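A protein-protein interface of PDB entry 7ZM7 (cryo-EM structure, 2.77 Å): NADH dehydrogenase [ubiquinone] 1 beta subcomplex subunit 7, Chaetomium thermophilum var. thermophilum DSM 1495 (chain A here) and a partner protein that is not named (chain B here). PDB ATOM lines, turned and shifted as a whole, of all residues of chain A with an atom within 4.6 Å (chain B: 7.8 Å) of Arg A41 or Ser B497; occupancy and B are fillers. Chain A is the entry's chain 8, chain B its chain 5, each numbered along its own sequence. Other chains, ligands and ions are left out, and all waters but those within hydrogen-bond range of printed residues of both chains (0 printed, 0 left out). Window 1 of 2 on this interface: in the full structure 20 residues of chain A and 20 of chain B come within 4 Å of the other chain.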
ATOM      1  N   PRO A  23     -22.638 -11.132 -25.559  1.00  0.00           N
ATOM      2  CA  PRO A  23     -23.074 -11.670 -24.269  1.00  0.00           C
ATOM      3  C   PRO A  23     -23.472 -10.568 -23.305  1.00  0.00           C
ATOM      4  O   PRO A  23     -22.942  -9.458 -23.339  1.00  0.00           O
ATOM      5  CB  PRO A  23     -21.845 -12.431 -23.774  1.00  0.00           C
ATOM      6  CG  PRO A  23     -21.109 -12.775 -25.001  1.00  0.00           C
ATOM      7  CD  PRO A  23     -21.306 -11.635 -25.927  1.00  0.00           C
ATOM      8  N   LEU A  34     -16.154  -5.500 -29.287  1.00  0.00           N
ATOM      9  CA  LEU A  34     -16.441  -6.921 -29.132  1.00  0.00           C
ATOM     10  C   LEU A  34     -17.152  -7.471 -30.350  1.00  0.00           C
ATOM     11  O   LEU A  34     -16.981  -8.645 -30.696  1.00  0.00           O
ATOM     12  CB  LEU A  34     -17.287  -7.173 -27.894  1.00  0.00           C
ATOM     13  CG  LEU A  34     -17.287  -8.621 -27.431  1.00  0.00           C
ATOM     14  CD1 LEU A  34     -15.898  -9.180 -27.406  1.00  0.00           C
ATOM     15  CD2 LEU A  34     -17.910  -8.705 -26.070  1.00  0.00           C
ATOM     16  N   LEU A  37     -14.396  -8.288 -32.646  1.00  0.00           N
ATOM     17  CA  LEU A  37     -13.604  -9.352 -32.047  1.00  0.00           C
ATOM     18  C   LEU A  37     -14.297 -10.693 -32.198  1.00  0.00           C
ATOM     19  O   LEU A  37     -13.713 -11.650 -32.711  1.00  0.00           O
ATOM     20  CB  LEU A  37     -13.342  -9.066 -30.576  1.00  0.00           C
ATOM     21  CG  LEU A  37     -12.713 -10.276 -29.887  1.00  0.00           C
ATOM     22  CD1 LEU A  37     -11.402 -10.656 -30.564  1.00  0.00           C
ATOM     23  CD2 LEU A  37     -12.508 -10.017 -28.414  1.00  0.00           C
ATOM     24  N   ASN A  38     -15.555 -10.777 -31.768  1.00  0.00           N
ATOM     25  CA  ASN A  38     -16.289 -12.029 -31.883  1.00  0.00           C
ATOM     26  C   ASN A  38     -16.458 -12.422 -33.343  1.00  0.00           C
ATOM     27  O   ASN A  38     -16.359 -13.600 -33.693  1.00  0.00           O
ATOM     28  CB  ASN A  38     -17.638 -11.893 -31.189  1.00  0.00           C
ATOM     29  CG  ASN A  38     -17.539 -12.058 -29.688  1.00  0.00           C
ATOM     30  OD1 ASN A  38     -16.472 -12.343 -29.151  1.00  0.00           O
ATOM     31  ND2 ASN A  38     -18.653 -11.855 -28.998  1.00  0.00           N
ATOM     32  N   ARG A  39     -16.710 -11.446 -34.211  1.00  0.00           N
ATOM     33  CA  ARG A  39     -16.810 -11.722 -35.637  1.00  0.00           C
ATOM     34  C   ARG A  39     -15.493 -12.237 -36.191  1.00  0.00           C
ATOM     35  O   ARG A  39     -15.476 -13.163 -37.007  1.00  0.00           O
ATOM     36  CB  ARG A  39     -17.246 -10.458 -36.378  1.00  0.00           C
ATOM     37  CG  ARG A  39     -17.416 -10.628 -37.871  1.00  0.00           C
ATOM     38  CD  ARG A  39     -18.570 -11.558 -38.175  1.00  0.00           C
ATOM     39  NE  ARG A  39     -18.789 -11.703 -39.609  1.00  0.00           N
ATOM     40  CZ  ARG A  39     -19.624 -12.582 -40.150  1.00  0.00           C
ATOM     41  NH1 ARG A  39     -20.320 -13.401 -39.375  1.00  0.00           N
ATOM     42  NH2 ARG A  39     -19.763 -12.643 -41.466  1.00  0.00           N
ATOM     43  N   CYS A  40     -14.378 -11.634 -35.781  1.00  0.00           N
ATOM     44  CA  CYS A  40     -13.075 -12.183 -36.132  1.00  0.00           C
ATOM     45  C   CYS A  40     -12.917 -13.577 -35.567  1.00  0.00           C
ATOM     46  O   CYS A  40     -12.413 -14.480 -36.243  1.00  0.00           O
ATOM     47  CB  CYS A  40     -11.952 -11.282 -35.619  1.00  0.00           C
ATOM     48  SG  CYS A  40     -10.284 -11.748 -36.175  1.00  0.00           S
ATOM     49  N   ARG A  41     -13.344 -13.775 -34.324  1.00  0.00           N
ATOM     50  CA  ARG A  41     -13.263 -15.093 -33.718  1.00  0.00           C
ATOM     51  C   ARG A  41     -14.122 -16.104 -34.458  1.00  0.00           C
ATOM     52  O   ARG A  41     -13.713 -17.258 -34.625  1.00  0.00           O
ATOM     53  CB  ARG A  41     -13.674 -15.009 -32.257  1.00  0.00           C
ATOM     54  CG  ARG A  41     -12.677 -14.323 -31.374  1.00  0.00           C
ATOM     55  CD  ARG A  41     -12.803 -14.849 -29.979  1.00  0.00           C
ATOM     56  NE  ARG A  41     -13.712 -14.052 -29.187  1.00  0.00           N
ATOM     57  CZ  ARG A  41     -13.370 -13.443 -28.067  1.00  0.00           C
ATOM     58  NH1 ARG A  41     -14.258 -12.724 -27.412  1.00  0.00           N
ATOM     59  NH2 ARG A  41     -12.130 -13.541 -27.619  1.00  0.00           N
ATOM     60  N   TYR A  42     -15.307 -15.698 -34.907  1.00  0.00           N
ATOM     61  CA  TYR A  42     -16.168 -16.609 -35.647  1.00  0.00           C
ATOM     62  C   TYR A  42     -15.520 -17.054 -36.947  1.00  0.00           C
ATOM     63  O   TYR A  42     -15.545 -18.243 -37.278  1.00  0.00           O
ATOM     64  CB  TYR A  42     -17.500 -15.929 -35.941  1.00  0.00           C
ATOM     65  CG  TYR A  42     -18.261 -16.496 -37.117  1.00  0.00           C
ATOM     66  CD1 TYR A  42     -19.068 -17.611 -36.969  1.00  0.00           C
ATOM     67  CD2 TYR A  42     -18.153 -15.930 -38.377  1.00  0.00           C
ATOM     68  CE1 TYR A  42     -19.766 -18.124 -38.027  1.00  0.00           C
ATOM     69  CE2 TYR A  42     -18.839 -16.448 -39.446  1.00  0.00           C
ATOM     70  CZ  TYR A  42     -19.639 -17.548 -39.267  1.00  0.00           C
ATOM     71  OH  TYR A  42     -20.326 -18.064 -40.333  1.00  0.00           O
ATOM     72  N   GLU A  43     -14.931 -16.121 -37.691  1.00  0.00           N
ATOM     73  CA  GLU A  43     -14.342 -16.434 -38.983  1.00  0.00           C
ATOM     74  C   GLU A  43     -13.060 -17.246 -38.877  1.00  0.00           C
ATOM     75  O   GLU A  43     -12.575 -17.737 -39.900  1.00  0.00           O
ATOM     76  CB  GLU A  43     -14.053 -15.149 -39.767  1.00  0.00           C
ATOM     77  CG  GLU A  43     -15.273 -14.498 -40.405  1.00  0.00           C
ATOM     78  CD  GLU A  43     -15.097 -13.003 -40.631  1.00  0.00           C
ATOM     79  OE1 GLU A  43     -14.741 -12.288 -39.671  1.00  0.00           O
ATOM     80  OE2 GLU A  43     -15.307 -12.546 -41.773  1.00  0.00           O
ATOM     81  N   THR A  44     -12.500 -17.400 -37.679  1.00  0.00           N
ATOM     82  CA  THR A  44     -11.197 -18.028 -37.513  1.00  0.00           C
ATOM     83  C   THR A  44     -11.243 -19.265 -36.640  1.00  0.00           C
ATOM     84  O   THR A  44     -10.192 -19.850 -36.369  1.00  0.00           O
ATOM     85  CB  THR A  44     -10.201 -17.033 -36.926  1.00  0.00           C
ATOM     86  OG1 THR A  44     -10.660 -16.613 -35.637  1.00  0.00           O
ATOM     87  CG2 THR A  44     -10.064 -15.825 -37.835  1.00  0.00           C
ATOM     88  N   TYR A  45     -12.434 -19.674 -36.202  1.00  0.00           N
ATOM     89  CA  TYR A  45     -12.646 -20.835 -35.330  1.00  0.00           C
ATOM     90  C   TYR A  45     -12.000 -20.672 -33.960  1.00  0.00           C
ATOM     91  O   TYR A  45     -11.569 -21.646 -33.352  1.00  0.00           O
ATOM     92  CB  TYR A  45     -12.161 -22.126 -35.980  1.00  0.00           C
ATOM     93  CG  TYR A  45     -13.100 -22.676 -37.014  1.00  0.00           C
ATOM     94  CD1 TYR A  45     -13.023 -22.264 -38.327  1.00  0.00           C
ATOM     95  CD2 TYR A  45     -14.045 -23.631 -36.681  1.00  0.00           C
ATOM     96  CE1 TYR A  45     -13.869 -22.768 -39.273  1.00  0.00           C
ATOM     97  CE2 TYR A  45     -14.895 -24.137 -37.620  1.00  0.00           C
ATOM     98  CZ  TYR A  45     -14.804 -23.705 -38.915  1.00  0.00           C
ATOM     99  OH  TYR A  45     -15.653 -24.216 -39.864  1.00  0.00           O
ATOM    100  N   TYR A  46     -11.991 -19.441 -33.449  1.00  0.00           N
ATOM    101  CA  TYR A  46     -11.469 -19.176 -32.079  1.00  0.00           C
ATOM    102  C   TYR A  46     -10.029 -19.671 -31.922  1.00  0.00           C
ATOM    103  O   TYR A  46      -9.678 -20.076 -30.800  1.00  0.00           O
ATOM    104  CB  TYR A  46     -12.352 -19.825 -31.005  1.00  0.00           C
ATOM    105  CG  TYR A  46     -13.760 -19.305 -30.876  1.00  0.00           C
ATOM    106  CD1 TYR A  46     -14.761 -19.725 -31.734  1.00  0.00           C
ATOM    107  CD2 TYR A  46     -14.102 -18.423 -29.865  1.00  0.00           C
ATOM    108  CE1 TYR A  46     -16.060 -19.261 -31.613  1.00  0.00           C
ATOM    109  CE2 TYR A  46     -15.396 -17.949 -29.729  1.00  0.00           C
ATOM    110  CZ  TYR A  46     -16.380 -18.371 -30.604  1.00  0.00           C
ATOM    111  OH  TYR A  46     -17.659 -17.912 -30.476  1.00  0.00           O
ATOM    112  N   CYS A  51      -6.583 -13.746 -34.443  1.00  0.00           N
ATOM    113  CA  CYS A  51      -7.182 -12.437 -34.210  1.00  0.00           C
ATOM    114  C   CYS A  51      -6.373 -11.646 -33.188  1.00  0.00           C
ATOM    115  O   CYS A  51      -6.922 -11.069 -32.249  1.00  0.00           O
ATOM    116  CB  CYS A  51      -8.632 -12.569 -33.755  1.00  0.00           C
ATOM    117  SG  CYS A  51      -9.737 -13.296 -34.972  1.00  0.00           S
ATOM    118  N   ARG A  55      -8.223  -8.790 -30.706  1.00  0.00           N
ATOM    119  CA  ARG A  55      -8.220  -9.119 -29.256  1.00  0.00           C
ATOM    120  C   ARG A  55      -7.527  -7.986 -28.500  1.00  0.00           C
ATOM    121  O   ARG A  55      -8.114  -7.485 -27.535  1.00  0.00           O
ATOM    122  CB  ARG A  55      -7.429 -10.402 -28.988  1.00  0.00           C
ATOM    123  CG  ARG A  55      -8.156 -11.686 -29.352  1.00  0.00           C
ATOM    124  CD  ARG A  55      -7.165 -12.819 -29.528  1.00  0.00           C
ATOM    125  NE  ARG A  55      -7.735 -13.888 -30.331  1.00  0.00           N
ATOM    126  CZ  ARG A  55      -8.279 -14.986 -29.829  1.00  0.00           C
ATOM    127  NH1 ARG A  55      -8.304 -15.165 -28.520  1.00  0.00           N
ATOM    128  NH2 ARG A  55      -8.778 -15.905 -30.635  1.00  0.00           N
ATOM    129  N   PHE B  52     -19.578 -24.188 -33.247  1.00  0.00           N
ATOM    130  CA  PHE B  52     -18.868 -23.227 -34.075  1.00  0.00           C
ATOM    131  C   PHE B  52     -19.789 -22.529 -35.058  1.00  0.00           C
ATOM    132  O   PHE B  52     -19.328 -21.712 -35.859  1.00  0.00           O
ATOM    133  CB  PHE B  52     -17.717 -23.907 -34.802  1.00  0.00           C
ATOM    134  CG  PHE B  52     -16.529 -24.137 -33.934  1.00  0.00           C
ATOM    135  CD1 PHE B  52     -15.789 -23.068 -33.469  1.00  0.00           C
ATOM    136  CD2 PHE B  52     -16.153 -25.410 -33.575  1.00  0.00           C
ATOM    137  CE1 PHE B  52     -14.693 -23.266 -32.664  1.00  0.00           C
ATOM    138  CE2 PHE B  52     -15.059 -25.612 -32.772  1.00  0.00           C
ATOM    139  CZ  PHE B  52     -14.328 -24.540 -32.316  1.00  0.00           C
ATOM    140  N   ASN B 323     -18.189 -20.770 -17.117  1.00  0.00           N
ATOM    141  CA  ASN B 323     -17.393 -21.174 -18.263  1.00  0.00           C
ATOM    142  C   ASN B 323     -16.000 -21.603 -17.839  1.00  0.00           C
ATOM    143  O   ASN B 323     -15.332 -22.344 -18.560  1.00  0.00           O
ATOM    144  CB  ASN B 323     -17.315 -20.043 -19.284  1.00  0.00           C
ATOM    145  CG  ASN B 323     -16.560 -18.842 -18.771  1.00  0.00           C
ATOM    146  OD1 ASN B 323     -16.344 -18.689 -17.572  1.00  0.00           O
ATOM    147  ND2 ASN B 323     -16.112 -18.000 -19.686  1.00  0.00           N
ATOM    148  N   THR B 488      -7.957 -24.385 -26.728  1.00  0.00           N
ATOM    149  CA  THR B 488      -9.354 -24.048 -26.498  1.00  0.00           C
ATOM    150  C   THR B 488      -9.529 -22.960 -25.451  1.00  0.00           C
ATOM    151  O   THR B 488     -10.663 -22.683 -25.041  1.00  0.00           O
ATOM    152  CB  THR B 488     -10.132 -25.301 -26.094  1.00  0.00           C
ATOM    153  OG1 THR B 488      -9.588 -25.830 -24.881  1.00  0.00           O
ATOM    154  CG2 THR B 488     -10.070 -26.351 -27.182  1.00  0.00           C
ATOM    155  N   LYS B 489      -8.444 -22.316 -25.027  1.00  0.00           N
ATOM    156  CA  LYS B 489      -8.539 -21.335 -23.953  1.00  0.00           C
ATOM    157  C   LYS B 489      -9.319 -20.103 -24.382  1.00  0.00           C
ATOM    158  O   LYS B 489      -9.654 -19.259 -23.547  1.00  0.00           O
ATOM    159  CB  LYS B 489      -7.145 -20.937 -23.479  1.00  0.00           C
ATOM    160  CG  LYS B 489      -6.541 -19.769 -24.232  1.00  0.00           C
ATOM    161  CD  LYS B 489      -5.174 -19.406 -23.677  1.00  0.00           C
ATOM    162  CE  LYS B 489      -4.610 -18.172 -24.354  1.00  0.00           C
ATOM    163  NZ  LYS B 489      -5.369 -16.946 -23.992  1.00  0.00           N
ATOM    164  N   ASP B 490      -9.588 -19.961 -25.671  1.00  0.00           N
ATOM    165  CA  ASP B 490     -10.408 -18.854 -26.127  1.00  0.00           C
ATOM    166  C   ASP B 490     -11.872 -19.240 -26.221  1.00  0.00           C
ATOM    167  O   ASP B 490     -12.744 -18.421 -25.925  1.00  0.00           O
ATOM    168  CB  ASP B 490      -9.893 -18.365 -27.474  1.00  0.00           C
ATOM    169  CG  ASP B 490     -10.661 -17.197 -27.993  1.00  0.00           C
ATOM    170  OD1 ASP B 490     -10.896 -16.253 -27.219  1.00  0.00           O
ATOM    171  OD2 ASP B 490     -11.025 -17.225 -29.177  1.00  0.00           O
ATOM    172  N   ILE B 491     -12.148 -20.483 -26.607  1.00  0.00           N
ATOM    173  CA  ILE B 491     -13.514 -20.975 -26.689  1.00  0.00           C
ATOM    174  C   ILE B 491     -14.219 -20.819 -25.354  1.00  0.00           C
ATOM    175  O   ILE B 491     -15.397 -20.455 -25.294  1.00  0.00           O
ATOM    176  CB  ILE B 491     -13.503 -22.442 -27.159  1.00  0.00           C
ATOM    177  CG1 ILE B 491     -12.920 -22.535 -28.556  1.00  0.00           C
ATOM    178  CG2 ILE B 491     -14.877 -23.066 -27.085  1.00  0.00           C
ATOM    179  CD1 ILE B 491     -12.628 -23.923 -28.996  1.00  0.00           C
ATOM    180  N   PHE B 492     -13.510 -21.085 -24.265  1.00  0.00           N
ATOM    181  CA  PHE B 492     -14.084 -21.144 -22.934  1.00  0.00           C
ATOM    182  C   PHE B 492     -13.788 -19.901 -22.109  1.00  0.00           C
ATOM    183  O   PHE B 492     -14.689 -19.364 -21.462  1.00  0.00           O
ATOM    184  CB  PHE B 492     -13.567 -22.388 -22.205  1.00  0.00           C
ATOM    185  CG  PHE B 492     -13.962 -23.680 -22.863  1.00  0.00           C
ATOM    186  CD1 PHE B 492     -13.290 -24.140 -23.973  1.00  0.00           C
ATOM    187  CD2 PHE B 492     -14.996 -24.436 -22.357  1.00  0.00           C
ATOM    188  CE1 PHE B 492     -13.656 -25.311 -24.573  1.00  0.00           C
ATOM    189  CE2 PHE B 492     -15.361 -25.616 -22.951  1.00  0.00           C
ATOM    190  CZ  PHE B 492     -14.693 -26.054 -24.062  1.00  0.00           C
ATOM    191  N   ILE B 493     -12.538 -19.445 -22.088  1.00  0.00           N
ATOM    192  CA  ILE B 493     -12.201 -18.280 -21.279  1.00  0.00           C
ATOM    193  C   ILE B 493     -12.390 -16.998 -22.074  1.00  0.00           C
ATOM    194  O   ILE B 493     -13.239 -16.167 -21.740  1.00  0.00           O
ATOM    195  CB  ILE B 493     -10.767 -18.391 -20.728  1.00  0.00           C
ATOM    196  CG1 ILE B 493     -10.447 -19.825 -20.315  1.00  0.00           C
ATOM    197  CG2 ILE B 493     -10.570 -17.449 -19.555  1.00  0.00           C
ATOM    198  CD1 ILE B 493     -11.360 -20.352 -19.232  1.00  0.00           C
ATOM    199  N   GLY B 494     -11.617 -16.830 -23.141  1.00  0.00           N
ATOM    200  CA  GLY B 494     -11.618 -15.624 -23.943  1.00  0.00           C
ATOM    201  C   GLY B 494     -11.554 -14.374 -23.090  1.00  0.00           C
ATOM    202  O   GLY B 494     -10.992 -14.356 -21.991  1.00  0.00           O
ATOM    203  N   LEU B 495     -12.125 -13.313 -23.608  1.00  0.00           N
ATOM    204  CA  LEU B 495     -12.437 -12.156 -22.783  1.00  0.00           C
ATOM    205  C   LEU B 495     -13.882 -11.724 -22.940  1.00  0.00           C
ATOM    206  O   LEU B 495     -14.509 -11.321 -21.960  1.00  0.00           O
ATOM    207  CB  LEU B 495     -11.512 -10.987 -23.108  1.00  0.00           C
ATOM    208  CG  LEU B 495     -11.698  -9.804 -22.161  1.00  0.00           C
ATOM    209  CD1 LEU B 495     -11.402 -10.224 -20.735  1.00  0.00           C
ATOM    210  CD2 LEU B 495     -10.821  -8.641 -22.568  1.00  0.00           C
ATOM    211  N   GLY B 496     -14.427 -11.811 -24.148  1.00  0.00           N
ATOM    212  CA  GLY B 496     -15.826 -11.531 -24.376  1.00  0.00           C
ATOM    213  C   GLY B 496     -16.423 -12.594 -25.262  1.00  0.00           C
ATOM    214  O   GLY B 496     -17.311 -12.329 -26.072  1.00  0.00           O
ATOM    215  N   SER B 497     -15.906 -13.806 -25.123  1.00  0.00           N
ATOM    216  CA  SER B 497     -16.224 -14.878 -26.048  1.00  0.00           C
ATOM    217  C   SER B 497     -17.704 -15.219 -26.003  1.00  0.00           C
ATOM    218  O   SER B 497     -18.344 -15.173 -24.949  1.00  0.00           O
ATOM    219  CB  SER B 497     -15.388 -16.104 -25.719  1.00  0.00           C
ATOM    220  OG  SER B 497     -15.702 -17.172 -26.584  1.00  0.00           O
ATOM    221  N   ASN B 498     -18.245 -15.566 -27.159  1.00  0.00           N
ATOM    222  CA  ASN B 498     -19.664 -15.835 -27.312  1.00  0.00           C
ATOM    223  C   ASN B 498     -19.919 -17.278 -27.736  1.00  0.00           C
ATOM    224  O   ASN B 498     -20.759 -17.544 -28.592  1.00  0.00           O
ATOM    225  CB  ASN B 498     -20.274 -14.866 -28.315  1.00  0.00           C
ATOM    226  CG  ASN B 498     -19.544 -14.876 -29.633  1.00  0.00           C
ATOM    227  OD1 ASN B 498     -18.379 -15.259 -29.700  1.00  0.00           O
ATOM    228  ND2 ASN B 498     -20.220 -14.450 -30.690  1.00  0.00           N
ATOM    229  N   PHE B 499     -19.229 -18.235 -27.119  1.00  0.00           N
ATOM    230  CA  PHE B 499     -19.512 -19.650 -27.455  1.00  0.00           C
ATOM    231  C   PHE B 499     -20.833 -20.046 -26.802  1.00  0.00           C
ATOM    232  O   PHE B 499     -21.715 -20.586 -27.500  1.00  0.00           O
ATOM    233  CB  PHE B 499     -18.387 -20.588 -27.021  1.00  0.00           C
ATOM    234  CG  PHE B 499     -18.298 -21.898 -27.761  1.00  0.00           C
ATOM    235  CD1 PHE B 499     -18.044 -21.928 -29.122  1.00  0.00           C
ATOM    236  CD2 PHE B 499     -18.429 -23.103 -27.093  1.00  0.00           C
ATOM    237  CE1 PHE B 499     -17.940 -23.133 -29.798  1.00  0.00           C
ATOM    238  CE2 PHE B 499     -18.336 -24.307 -27.771  1.00  0.00           C
ATOM    239  CZ  PHE B 499     -18.090 -24.320 -29.122  1.00  0.00           C
ATOM    240  N   PHE B 500     -20.961 -19.789 -25.505  1.00  0.00           N
ATOM    241  CA  PHE B 500     -22.203 -20.139 -24.779  1.00  0.00           C
ATOM    242  C   PHE B 500     -23.176 -18.952 -24.824  1.00  0.00           C
ATOM    243  O   PHE B 500     -23.473 -18.406 -23.751  1.00  0.00           O
ATOM    244  CB  PHE B 500     -21.811 -20.650 -23.388  1.00  0.00           C
ATOM    245  CG  PHE B 500     -20.547 -21.471 -23.390  1.00  0.00           C
ATOM    246  CD1 PHE B 500     -20.569 -22.805 -23.763  1.00  0.00           C
ATOM    247  CD2 PHE B 500     -19.329 -20.905 -23.049  1.00  0.00           C
ATOM    248  CE1 PHE B 500     -19.403 -23.554 -23.790  1.00  0.00           C
ATOM    249  CE2 PHE B 500     -18.165 -21.656 -23.072  1.00  0.00           C
ATOM    250  CZ  PHE B 500     -18.204 -22.978 -23.445  1.00  0.00           C
ATOM    251  N   VAL B 501     -23.673 -18.582 -26.010  1.00  0.00           N
ATOM    252  CA  VAL B 501     -24.591 -17.407 -26.170  1.00  0.00           C
ATOM    253  C   VAL B 501     -26.019 -17.894 -26.412  1.00  0.00           C
ATOM    254  O   VAL B 501     -26.881 -17.077 -26.771  1.00  0.00           O
ATOM    255  CB  VAL B 501     -24.085 -16.466 -27.274  1.00  0.00           C
ATOM    256  CG1 VAL B 501     -24.415 -16.957 -28.677  1.00  0.00           C
ATOM    257  CG2 VAL B 501     -24.532 -15.034 -27.060  1.00  0.00           C
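Printed residues of chain B within 4 Å of Arg A41: Asp B490 (3.0 Å), Gly B496 (3.1 Å) and Ser B497 (3.0 Å).
Printed residues of chain A within 4 Å of Gly B496: Pro A23, Leu A34, Asn A38 and Arg A41.
Printed residues of chain B within 4 Å of Tyr A46: Phe B52, Asp B490, Ile B491, Ser B497, Asn B498 and Phe B499.
Of the printed residues of chain A, Ile B491 touches Tyr A46 (3.7 Å).
Thr A44 touches none of the printed residues of chain B.
The nearest printed residue of chain A that does not touch Ser B497 is Asn A38 (4.01 Å).
The nearest printed residue of chain B that does not touch Asn A38 is Ser B497 (4.01 Å).
Among the printed residues, merely in contact across the chains: Pro A23 with Gly B496, Pro A23 with Ser B497, Leu A34 with Gly B496, Tyr A45 with Phe B52, Tyr A46 with Phe B52, Tyr A46 with Asp B490, Tyr A46 with Ile B491, Tyr A46 with Ser B497 and Tyr A46 with Phe B499.
O of Asp B490 sits at hydrogen-bond distance from OG of Ser B497.
NH1 of Arg A41 sits at hydrogen-bond distance from OD1 of Asn A38.
The backbone carbonyl oxygen of Arg A41 lies within hydrogen-bond range of the side-chain hydroxyl of Thr A44 (3.3 Å).
The backbone carbonyl oxygen (O) of Arg A41 lies within hydrogen-bond range of the backbone NH (N) of Tyr A46, at 3.0 Å.
The side-chain sulfur (SG) of Cys A51 is in hydrogen-bond range of the backbone NH (N) of Arg A41.
The side-chain sulfur (SG) of Cys A40 forms a disulfide with the side-chain sulfur (SG) of Cys A51 (2.0 Å).
Of the 14 printed residues of chain A, 7 touch a printed residue of chain B.
Printed residues of chain A that touch a printed residue of chain B: Pro A23, Leu A34, Asn A38, Arg A41, Tyr A45, Tyr A46 and Arg A55.
Printed residues of chain B that touch a printed residue of chain A: Phe B52, Asp B490, Ile B491, Gly B496, Ser B497, Asn B498 and Phe B499.
Hydrophobic or aromatic side chains of chain B within 4 Å of the printed part of chain A: Phe B52 and Ile B491.
Among the printed residues, 16 pairs touch across the chains.
The guanidinium group (NH2) of Arg A41 lies within salt-bridge range of the side-chain carboxylate (OD1) of Asp B490, 3.0 Å away.
The side-chain carboxylate of Asp B490 lies within salt-bridge range of the guanidinium group of Arg A55 (3.0 Å).
The backbone carbonyl oxygen (O) of Gly B496 sits close to the side-chain amide oxygen (OD1) of Asn A38, at 3.2 Å.
O of Gly B496 lies close to NH1 of Arg A41 (3.4 Å).
The side-chain amide nitrogen (ND2) of Asn B498 lies close to the side-chain amide nitrogen (ND2) of Asn A38 (3.5 Å).
The side-chain amide oxygen (OD1) of Asn B498 lies within hydrogen-bond range of the side-chain hydroxyl (OH) of Tyr A46 (2.9 Å).
The guanidinium group (NH1) of Arg A41 lies close to the backbone NH (N) of Ser B497, at 3.0 Å.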
